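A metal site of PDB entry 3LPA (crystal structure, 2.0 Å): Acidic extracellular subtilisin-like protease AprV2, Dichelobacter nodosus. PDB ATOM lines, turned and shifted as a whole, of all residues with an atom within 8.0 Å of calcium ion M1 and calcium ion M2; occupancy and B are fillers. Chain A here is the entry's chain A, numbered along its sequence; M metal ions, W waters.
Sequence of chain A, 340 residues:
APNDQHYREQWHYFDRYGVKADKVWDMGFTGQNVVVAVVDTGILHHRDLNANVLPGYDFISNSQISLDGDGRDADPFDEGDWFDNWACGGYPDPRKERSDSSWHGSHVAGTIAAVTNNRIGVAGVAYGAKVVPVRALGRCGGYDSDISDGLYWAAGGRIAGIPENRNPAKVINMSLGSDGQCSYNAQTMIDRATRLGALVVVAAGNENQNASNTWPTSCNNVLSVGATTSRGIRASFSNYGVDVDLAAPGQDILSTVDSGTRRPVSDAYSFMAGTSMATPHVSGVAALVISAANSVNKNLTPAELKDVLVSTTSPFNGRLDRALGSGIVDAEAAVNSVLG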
ATOM      1  N   TYR A  57     -23.159 -26.302  26.762  1.00  0.00           N
ATOM      2  CA  TYR A  57     -22.731 -27.125  25.639  1.00  0.00           C
ATOM      3  C   TYR A  57     -23.721 -27.026  24.496  1.00  0.00           C
ATOM      4  O   TYR A  57     -24.901 -26.773  24.710  1.00  0.00           O
ATOM      5  CB  TYR A  57     -22.526 -28.595  26.059  1.00  0.00           C
ATOM      6  CG  TYR A  57     -21.510 -29.312  25.180  1.00  0.00           C
ATOM      7  CD1 TYR A  57     -20.149 -29.234  25.452  1.00  0.00           C
ATOM      8  CD2 TYR A  57     -21.918 -30.051  24.057  1.00  0.00           C
ATOM      9  CE1 TYR A  57     -19.212 -29.865  24.644  1.00  0.00           C
ATOM     10  CE2 TYR A  57     -20.967 -30.679  23.232  1.00  0.00           C
ATOM     11  CZ  TYR A  57     -19.630 -30.585  23.541  1.00  0.00           C
ATOM     12  OH  TYR A  57     -18.699 -31.205  22.753  1.00  0.00           O
ATOM     13  N   ASP A  58     -23.241 -27.256  23.277  1.00  0.00           N
ATOM     14  CA  ASP A  58     -24.065 -27.129  22.093  1.00  0.00           C
ATOM     15  C   ASP A  58     -24.343 -28.518  21.561  1.00  0.00           C
ATOM     16  O   ASP A  58     -23.451 -29.162  20.987  1.00  0.00           O
ATOM     17  CB  ASP A  58     -23.322 -26.297  21.047  1.00  0.00           C
ATOM     18  CG  ASP A  58     -24.208 -25.877  19.899  1.00  0.00           C
ATOM     19  OD1 ASP A  58     -25.174 -26.596  19.553  1.00  0.00           O
ATOM     20  OD2 ASP A  58     -23.917 -24.804  19.303  1.00  0.00           O
ATOM     21  N   PHE A  59     -25.581 -28.963  21.716  1.00  0.00           N
ATOM     22  CA  PHE A  59     -25.940 -30.326  21.313  1.00  0.00           C
ATOM     23  C   PHE A  59     -26.456 -30.451  19.893  1.00  0.00           C
ATOM     24  O   PHE A  59     -26.766 -31.552  19.442  1.00  0.00           O
ATOM     25  CB  PHE A  59     -26.918 -30.940  22.330  1.00  0.00           C
ATOM     26  CG  PHE A  59     -26.237 -31.421  23.562  1.00  0.00           C
ATOM     27  CD1 PHE A  59     -25.825 -32.748  23.671  1.00  0.00           C
ATOM     28  CD2 PHE A  59     -25.930 -30.549  24.578  1.00  0.00           C
ATOM     29  CE1 PHE A  59     -25.159 -33.181  24.799  1.00  0.00           C
ATOM     30  CE2 PHE A  59     -25.242 -30.993  25.722  1.00  0.00           C
ATOM     31  CZ  PHE A  59     -24.865 -32.291  25.826  1.00  0.00           C
ATOM     32  N   ILE A  60     -26.522 -29.339  19.157  1.00  0.00           N
ATOM     33  CA  ILE A  60     -27.110 -29.398  17.809  1.00  0.00           C
ATOM     34  C   ILE A  60     -26.150 -30.149  16.903  1.00  0.00           C
ATOM     35  O   ILE A  60     -24.991 -29.743  16.774  1.00  0.00           O
ATOM     36  CB  ILE A  60     -27.420 -27.999  17.215  1.00  0.00           C
ATOM     37  CG1 ILE A  60     -28.419 -27.220  18.106  1.00  0.00           C
ATOM     38  CG2 ILE A  60     -27.963 -28.144  15.798  1.00  0.00           C
ATOM     39  CD1 ILE A  60     -28.525 -25.701  17.772  1.00  0.00           C
ATOM     40  N   SER A  61     -26.639 -31.203  16.252  1.00  0.00           N
ATOM     41  CA  SER A  61     -25.769 -32.077  15.438  1.00  0.00           C
ATOM     42  C   SER A  61     -25.712 -31.680  13.970  1.00  0.00           C
ATOM     43  O   SER A  61     -24.630 -31.767  13.359  1.00  0.00           O
ATOM     44  CB  SER A  61     -26.184 -33.553  15.568  1.00  0.00           C
ATOM     45  OG  SER A  61     -26.063 -33.991  16.911  1.00  0.00           O
ATOM     46  N   ASN A  62     -26.851 -31.260  13.415  1.00  0.00           N
ATOM     47  CA  ASN A  62     -26.943 -30.728  12.028  1.00  0.00           C
ATOM     48  C   ASN A  62     -26.432 -29.278  11.915  1.00  0.00           C
ATOM     49  O   ASN A  62     -26.964 -28.381  12.524  1.00  0.00           O
ATOM     50  CB  ASN A  62     -28.404 -30.780  11.566  1.00  0.00           C
ATOM     51  CG  ASN A  62     -28.549 -30.640  10.055  1.00  0.00           C
ATOM     52  OD1 ASN A  62     -27.774 -29.937   9.386  1.00  0.00           O
ATOM     53  ND2 ASN A  62     -29.564 -31.281   9.522  1.00  0.00           N
ATOM     54  N   SER A  63     -25.407 -29.055  11.096  1.00  0.00           N
ATOM     55  CA  SER A  63     -24.779 -27.730  10.997  1.00  0.00           C
ATOM     56  C   SER A  63     -25.674 -26.740  10.243  1.00  0.00           C
ATOM     57  O   SER A  63     -25.465 -25.528  10.300  1.00  0.00           O
ATOM     58  CB  SER A  63     -23.440 -27.846  10.296  1.00  0.00           C
ATOM     59  OG  SER A  63     -23.609 -28.497   9.028  1.00  0.00           O
ATOM     60  N   ILE A  65     -28.743 -26.525  11.022  1.00  0.00           N
ATOM     61  CA  ILE A  65     -29.624 -26.025  12.104  1.00  0.00           C
ATOM     62  C   ILE A  65     -28.834 -25.082  13.028  1.00  0.00           C
ATOM     63  O   ILE A  65     -29.306 -23.975  13.381  1.00  0.00           O
ATOM     64  CB  ILE A  65     -30.314 -27.213  12.873  1.00  0.00           C
ATOM     65  CG1 ILE A  65     -31.200 -27.992  11.908  1.00  0.00           C
ATOM     66  CG2 ILE A  65     -31.147 -26.717  14.037  1.00  0.00           C
ATOM     67  CD1 ILE A  65     -31.845 -29.249  12.484  1.00  0.00           C
ATOM     68  N   SER A  66     -27.623 -25.518  13.389  1.00  0.00           N
ATOM     69  CA  SER A  66     -26.801 -24.785  14.353  1.00  0.00           C
ATOM     70  C   SER A  66     -26.290 -23.434  13.832  1.00  0.00           C
ATOM     71  O   SER A  66     -26.141 -22.489  14.613  1.00  0.00           O
ATOM     72  CB  SER A  66     -25.612 -25.648  14.826  1.00  0.00           C
ATOM     73  OG  SER A  66     -24.641 -25.836  13.811  1.00  0.00           O
ATOM     74  N   LEU A  67     -26.024 -23.368  12.537  1.00  0.00           N
ATOM     75  CA  LEU A  67     -25.486 -22.162  11.879  1.00  0.00           C
ATOM     76  C   LEU A  67     -24.174 -21.678  12.480  1.00  0.00           C
ATOM     77  O   LEU A  67     -23.878 -20.477  12.435  1.00  0.00           O
ATOM     78  CB  LEU A  67     -26.531 -21.044  11.826  1.00  0.00           C
ATOM     79  CG  LEU A  67     -27.800 -21.384  11.013  1.00  0.00           C
ATOM     80  CD1 LEU A  67     -28.826 -20.263  11.115  1.00  0.00           C
ATOM     81  CD2 LEU A  67     -27.443 -21.678   9.558  1.00  0.00           C
ATOM     82  N   ASP A  68     -23.396 -22.607  13.031  1.00  0.00           N
ATOM     83  CA  ASP A  68     -22.072 -22.307  13.587  1.00  0.00           C
ATOM     84  C   ASP A  68     -20.948 -23.050  12.862  1.00  0.00           C
ATOM     85  O   ASP A  68     -19.780 -22.934  13.276  1.00  0.00           O
ATOM     86  CB  ASP A  68     -22.019 -22.557  15.112  1.00  0.00           C
ATOM     87  CG  ASP A  68     -22.190 -24.027  15.506  1.00  0.00           C
ATOM     88  OD1 ASP A  68     -22.421 -24.905  14.639  1.00  0.00           O
ATOM     89  OD2 ASP A  68     -22.101 -24.330  16.719  1.00  0.00           O
ATOM     90  N   GLY A  69     -21.280 -23.816  11.817  1.00  0.00           N
ATOM     91  CA  GLY A  69     -20.268 -24.507  10.976  1.00  0.00           C
ATOM     92  C   GLY A  69     -19.892 -25.953  11.311  1.00  0.00           C
ATOM     93  O   GLY A  69     -19.131 -26.604  10.555  1.00  0.00           O
ATOM     94  N   ASP A  70     -20.420 -26.467  12.424  1.00  0.00           N
ATOM     95  CA  ASP A  70     -20.143 -27.843  12.851  1.00  0.00           C
ATOM     96  C   ASP A  70     -21.286 -28.432  13.712  1.00  0.00           C
ATOM     97  O   ASP A  70     -22.239 -27.721  14.031  1.00  0.00           O
ATOM     98  CB  ASP A  70     -18.786 -27.932  13.576  1.00  0.00           C
ATOM     99  CG  ASP A  70     -18.715 -27.089  14.874  1.00  0.00           C
ATOM    100  OD1 ASP A  70     -19.752 -26.508  15.295  1.00  0.00           O
ATOM    101  OD2 ASP A  70     -17.629 -27.023  15.512  1.00  0.00           O
ATOM    102  N   GLY A  71     -21.186 -29.713  14.066  1.00  0.00           N
ATOM    103  CA  GLY A  71     -22.146 -30.366  14.957  1.00  0.00           C
ATOM    104  C   GLY A  71     -21.855 -30.013  16.408  1.00  0.00           C
ATOM    105  O   GLY A  71     -21.563 -28.860  16.722  1.00  0.00           O
ATOM    106  N   ARG A  72     -21.863 -31.009  17.281  1.00  0.00           N
ATOM    107  CA  ARG A  72     -21.696 -30.750  18.710  1.00  0.00           C
ATOM    108  C   ARG A  72     -20.364 -30.083  19.043  1.00  0.00           C
ATOM    109  O   ARG A  72     -19.311 -30.509  18.600  1.00  0.00           O
ATOM    110  CB  ARG A  72     -21.929 -32.036  19.512  1.00  0.00           C
ATOM    111  CG  ARG A  72     -23.398 -32.443  19.474  1.00  0.00           C
ATOM    112  CD  ARG A  72     -23.720 -33.726  20.230  1.00  0.00           C
ATOM    113  NE  ARG A  72     -25.160 -33.975  20.144  1.00  0.00           N
ATOM    114  CZ  ARG A  72     -25.776 -35.076  20.565  1.00  0.00           C
ATOM    115  NH1 ARG A  72     -25.100 -36.078  21.113  1.00  0.00           N
ATOM    116  NH2 ARG A  72     -27.094 -35.163  20.442  1.00  0.00           N
ATOM    117  N   ASP A  73     -20.446 -29.022  19.830  1.00  0.00           N
ATOM    118  CA  ASP A  73     -19.263 -28.248  20.198  1.00  0.00           C
ATOM    119  C   ASP A  73     -19.473 -27.666  21.587  1.00  0.00           C
ATOM    120  O   ASP A  73     -20.560 -27.730  22.118  1.00  0.00           O
ATOM    121  CB  ASP A  73     -19.003 -27.126  19.188  1.00  0.00           C
ATOM    122  CG  ASP A  73     -20.086 -26.080  19.198  1.00  0.00           C
ATOM    123  OD1 ASP A  73     -21.093 -26.242  18.481  1.00  0.00           O
ATOM    124  OD2 ASP A  73     -19.936 -25.076  19.921  1.00  0.00           O
ATOM    125  N   ALA A  74     -18.418 -27.090  22.166  1.00  0.00           N
ATOM    126  CA  ALA A  74     -18.479 -26.624  23.544  1.00  0.00           C
ATOM    127  C   ALA A  74     -19.080 -25.231  23.719  1.00  0.00           C
ATOM    128  O   ALA A  74     -19.220 -24.749  24.840  1.00  0.00           O
ATOM    129  CB  ALA A  74     -17.074 -26.681  24.192  1.00  0.00           C
ATOM    130  N   ASP A  75     -19.436 -24.576  22.619  1.00  0.00           N
ATOM    131  CA  ASP A  75     -19.927 -23.200  22.740  1.00  0.00           C
ATOM    132  C   ASP A  75     -21.421 -23.096  22.435  1.00  0.00           C
ATOM    133  O   ASP A  75     -21.836 -23.206  21.270  1.00  0.00           O
ATOM    134  CB  ASP A  75     -19.091 -22.246  21.882  1.00  0.00           C
ATOM    135  CG  ASP A  75     -19.585 -20.790  21.952  1.00  0.00           C
ATOM    136  OD1 ASP A  75     -20.473 -20.463  22.764  1.00  0.00           O
ATOM    137  OD2 ASP A  75     -19.044 -19.975  21.172  1.00  0.00           O
ATOM    138  N   PRO A  76     -22.243 -22.867  23.487  1.00  0.00           N
ATOM    139  CA  PRO A  76     -23.701 -22.840  23.340  1.00  0.00           C
ATOM    140  C   PRO A  76     -24.256 -21.473  22.922  1.00  0.00           C
ATOM    141  O   PRO A  76     -25.400 -21.141  23.235  1.00  0.00           O
ATOM    142  CB  PRO A  76     -24.189 -23.185  24.745  1.00  0.00           C
ATOM    143  CG  PRO A  76     -23.215 -22.488  25.635  1.00  0.00           C
ATOM    144  CD  PRO A  76     -21.853 -22.515  24.873  1.00  0.00           C
ATOM    145  N   PHE A  77     -23.456 -20.701  22.207  1.00  0.00           N
ATOM    146  CA  PHE A  77     -23.849 -19.375  21.734  1.00  0.00           C
ATOM    147  C   PHE A  77     -25.049 -19.475  20.796  1.00  0.00           C
ATOM    148  O   PHE A  77     -25.054 -20.303  19.885  1.00  0.00           O
ATOM    149  CB  PHE A  77     -22.680 -18.720  20.989  1.00  0.00           C
ATOM    150  CG  PHE A  77     -22.948 -17.326  20.490  1.00  0.00           C
ATOM    151  CD1 PHE A  77     -23.255 -16.297  21.392  1.00  0.00           C
ATOM    152  CD2 PHE A  77     -22.850 -17.032  19.120  1.00  0.00           C
ATOM    153  CE1 PHE A  77     -23.505 -14.991  20.919  1.00  0.00           C
ATOM    154  CE2 PHE A  77     -23.075 -15.737  18.642  1.00  0.00           C
ATOM    155  CZ  PHE A  77     -23.406 -14.708  19.540  1.00  0.00           C
ATOM    156  N   ASP A  78     -26.048 -18.630  21.033  1.00  0.00           N
ATOM    157  CA  ASP A  78     -27.183 -18.550  20.126  1.00  0.00           C
ATOM    158  C   ASP A  78     -26.795 -17.758  18.906  1.00  0.00           C
ATOM    159  O   ASP A  78     -26.772 -16.525  18.944  1.00  0.00           O
ATOM    160  CB  ASP A  78     -28.423 -17.914  20.786  1.00  0.00           C
ATOM    161  CG  ASP A  78     -29.674 -18.110  19.943  1.00  0.00           C
ATOM    162  OD1 ASP A  78     -29.544 -18.538  18.759  1.00  0.00           O
ATOM    163  OD2 ASP A  78     -30.800 -17.898  20.473  1.00  0.00           O
ATOM    164  N   GLU A  79     -26.506 -18.470  17.814  1.00  0.00           N
ATOM    165  CA  GLU A  79     -26.161 -17.821  16.534  1.00  0.00           C
ATOM    166  C   GLU A  79     -27.348 -17.045  15.941  1.00  0.00           C
ATOM    167  O   GLU A  79     -27.155 -16.108  15.161  1.00  0.00           O
ATOM    168  CB  GLU A  79     -25.685 -18.853  15.490  1.00  0.00           C
ATOM    169  CG  GLU A  79     -24.645 -19.839  15.967  1.00  0.00           C
ATOM    170  CD  GLU A  79     -23.243 -19.235  16.173  1.00  0.00           C
ATOM    171  OE1 GLU A  79     -22.934 -18.148  15.632  1.00  0.00           O
ATOM    172  OE2 GLU A  79     -22.442 -19.858  16.869  1.00  0.00           O
ATOM    173  N   ARG A 135     -27.608 -25.835  24.423  1.00  0.00           N
ATOM    174  CA  ARG A 135     -28.138 -25.467  23.104  1.00  0.00           C
ATOM    175  C   ARG A 135     -28.543 -26.709  22.309  1.00  0.00           C
ATOM    176  O   ARG A 135     -27.690 -27.501  21.902  1.00  0.00           O
ATOM    177  CB  ARG A 135     -27.149 -24.608  22.315  1.00  0.00           C
ATOM    178  CG  ARG A 135     -27.739 -24.001  21.023  1.00  0.00           C
ATOM    179  CD  ARG A 135     -26.654 -23.235  20.225  1.00  0.00           C
ATOM    180  NE  ARG A 135     -27.200 -22.440  19.110  1.00  0.00           N
ATOM    181  CZ  ARG A 135     -26.758 -22.473  17.856  1.00  0.00           C
ATOM    182  NH1 ARG A 135     -25.742 -23.234  17.539  1.00  0.00           N
ATOM    183  NH2 ARG A 135     -27.356 -21.711  16.918  1.00  0.00           N
HETATM  184 CA    CA M   1     -21.885 -26.723  16.299  1.00  0.00          CA
HETATM  185 CA    CA M   2     -21.872 -23.742  19.031  1.00  0.00          CA
HETATM  186  O   HOH W   1     -20.022 -22.564  18.169  1.00  0.00           O
HETATM  187  O   HOH W   2     -23.995 -27.327  17.119  1.00  0.00           O
HETATM  188  O   HOH W   3     -22.713 -21.777  18.693  1.00  0.00           O
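Water W2 bridges the backbone carbonyl oxygen of Ile 60 (2.6 Å) and the side-chain carboxylate of Asp 58 (2.8 Å). Water W3 lies within hydrogen-bond range of the side-chain carboxylate (OE2) of Glu 79 (2.7 Å) and the backbone carbonyl oxygen (O) of Phe 77 (3.0 Å).
N of Ile 60 is in hydrogen-bond range of OD1 of Asp 58, 3.1 Å away. The side-chain carboxylate (OD1) of Asp 68 lies close to the side-chain hydroxyl (OG) of Ser 66, at 2.5 Å. NH1 of Arg 135 sits close to OD2 of Asp 68 (3.9 Å). The guanidinium group of Arg 135 is in salt-bridge range of the side-chain carboxylate of Asp 58 (3.96 Å). The backbone carbonyl oxygen (O) of Ser 66 is in hydrogen-bond range of the guanidinium group (NH2) of Arg 135, at 2.7 Å. OG of Ser 66 sits close to O of Asp 70, 3.1 Å away. N of Phe 77 lies within hydrogen-bond range of OD1 of Asp 75, at 3.0 Å.
Calcium ion M2 is bound by water W3, the backbone carbonyl oxygen (O) of Asp 75, the side-chain carboxylate (OD2) of Asp 58, water W1, the side-chain carboxylate (OD2) of Asp 68, the side-chain carboxylate (OD2) of Asp 73 and the side-chain carboxylate (OD1) of Asp 73.
The backbone carbonyl oxygen (O) of Gly 71 binds calcium ion M1 (2.2 Å). Water W2 binds calcium ion M1, 2.3 Å away. OD1 of Asp 70 binds calcium ion M1, 2.4 Å away. OD1 of Asp 73 binds calcium ion M1, at 2.4 Å. OD2 of Asp 68 binds calcium ion M1 (2.4 Å). O of Asp 70 binds calcium ion M1 (2.5 Å). OD1 of Asp 68 binds calcium ion M1 (2.5 Å).
Residues that only touch calcium ion M1: Ser 66 (3.8 Å).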
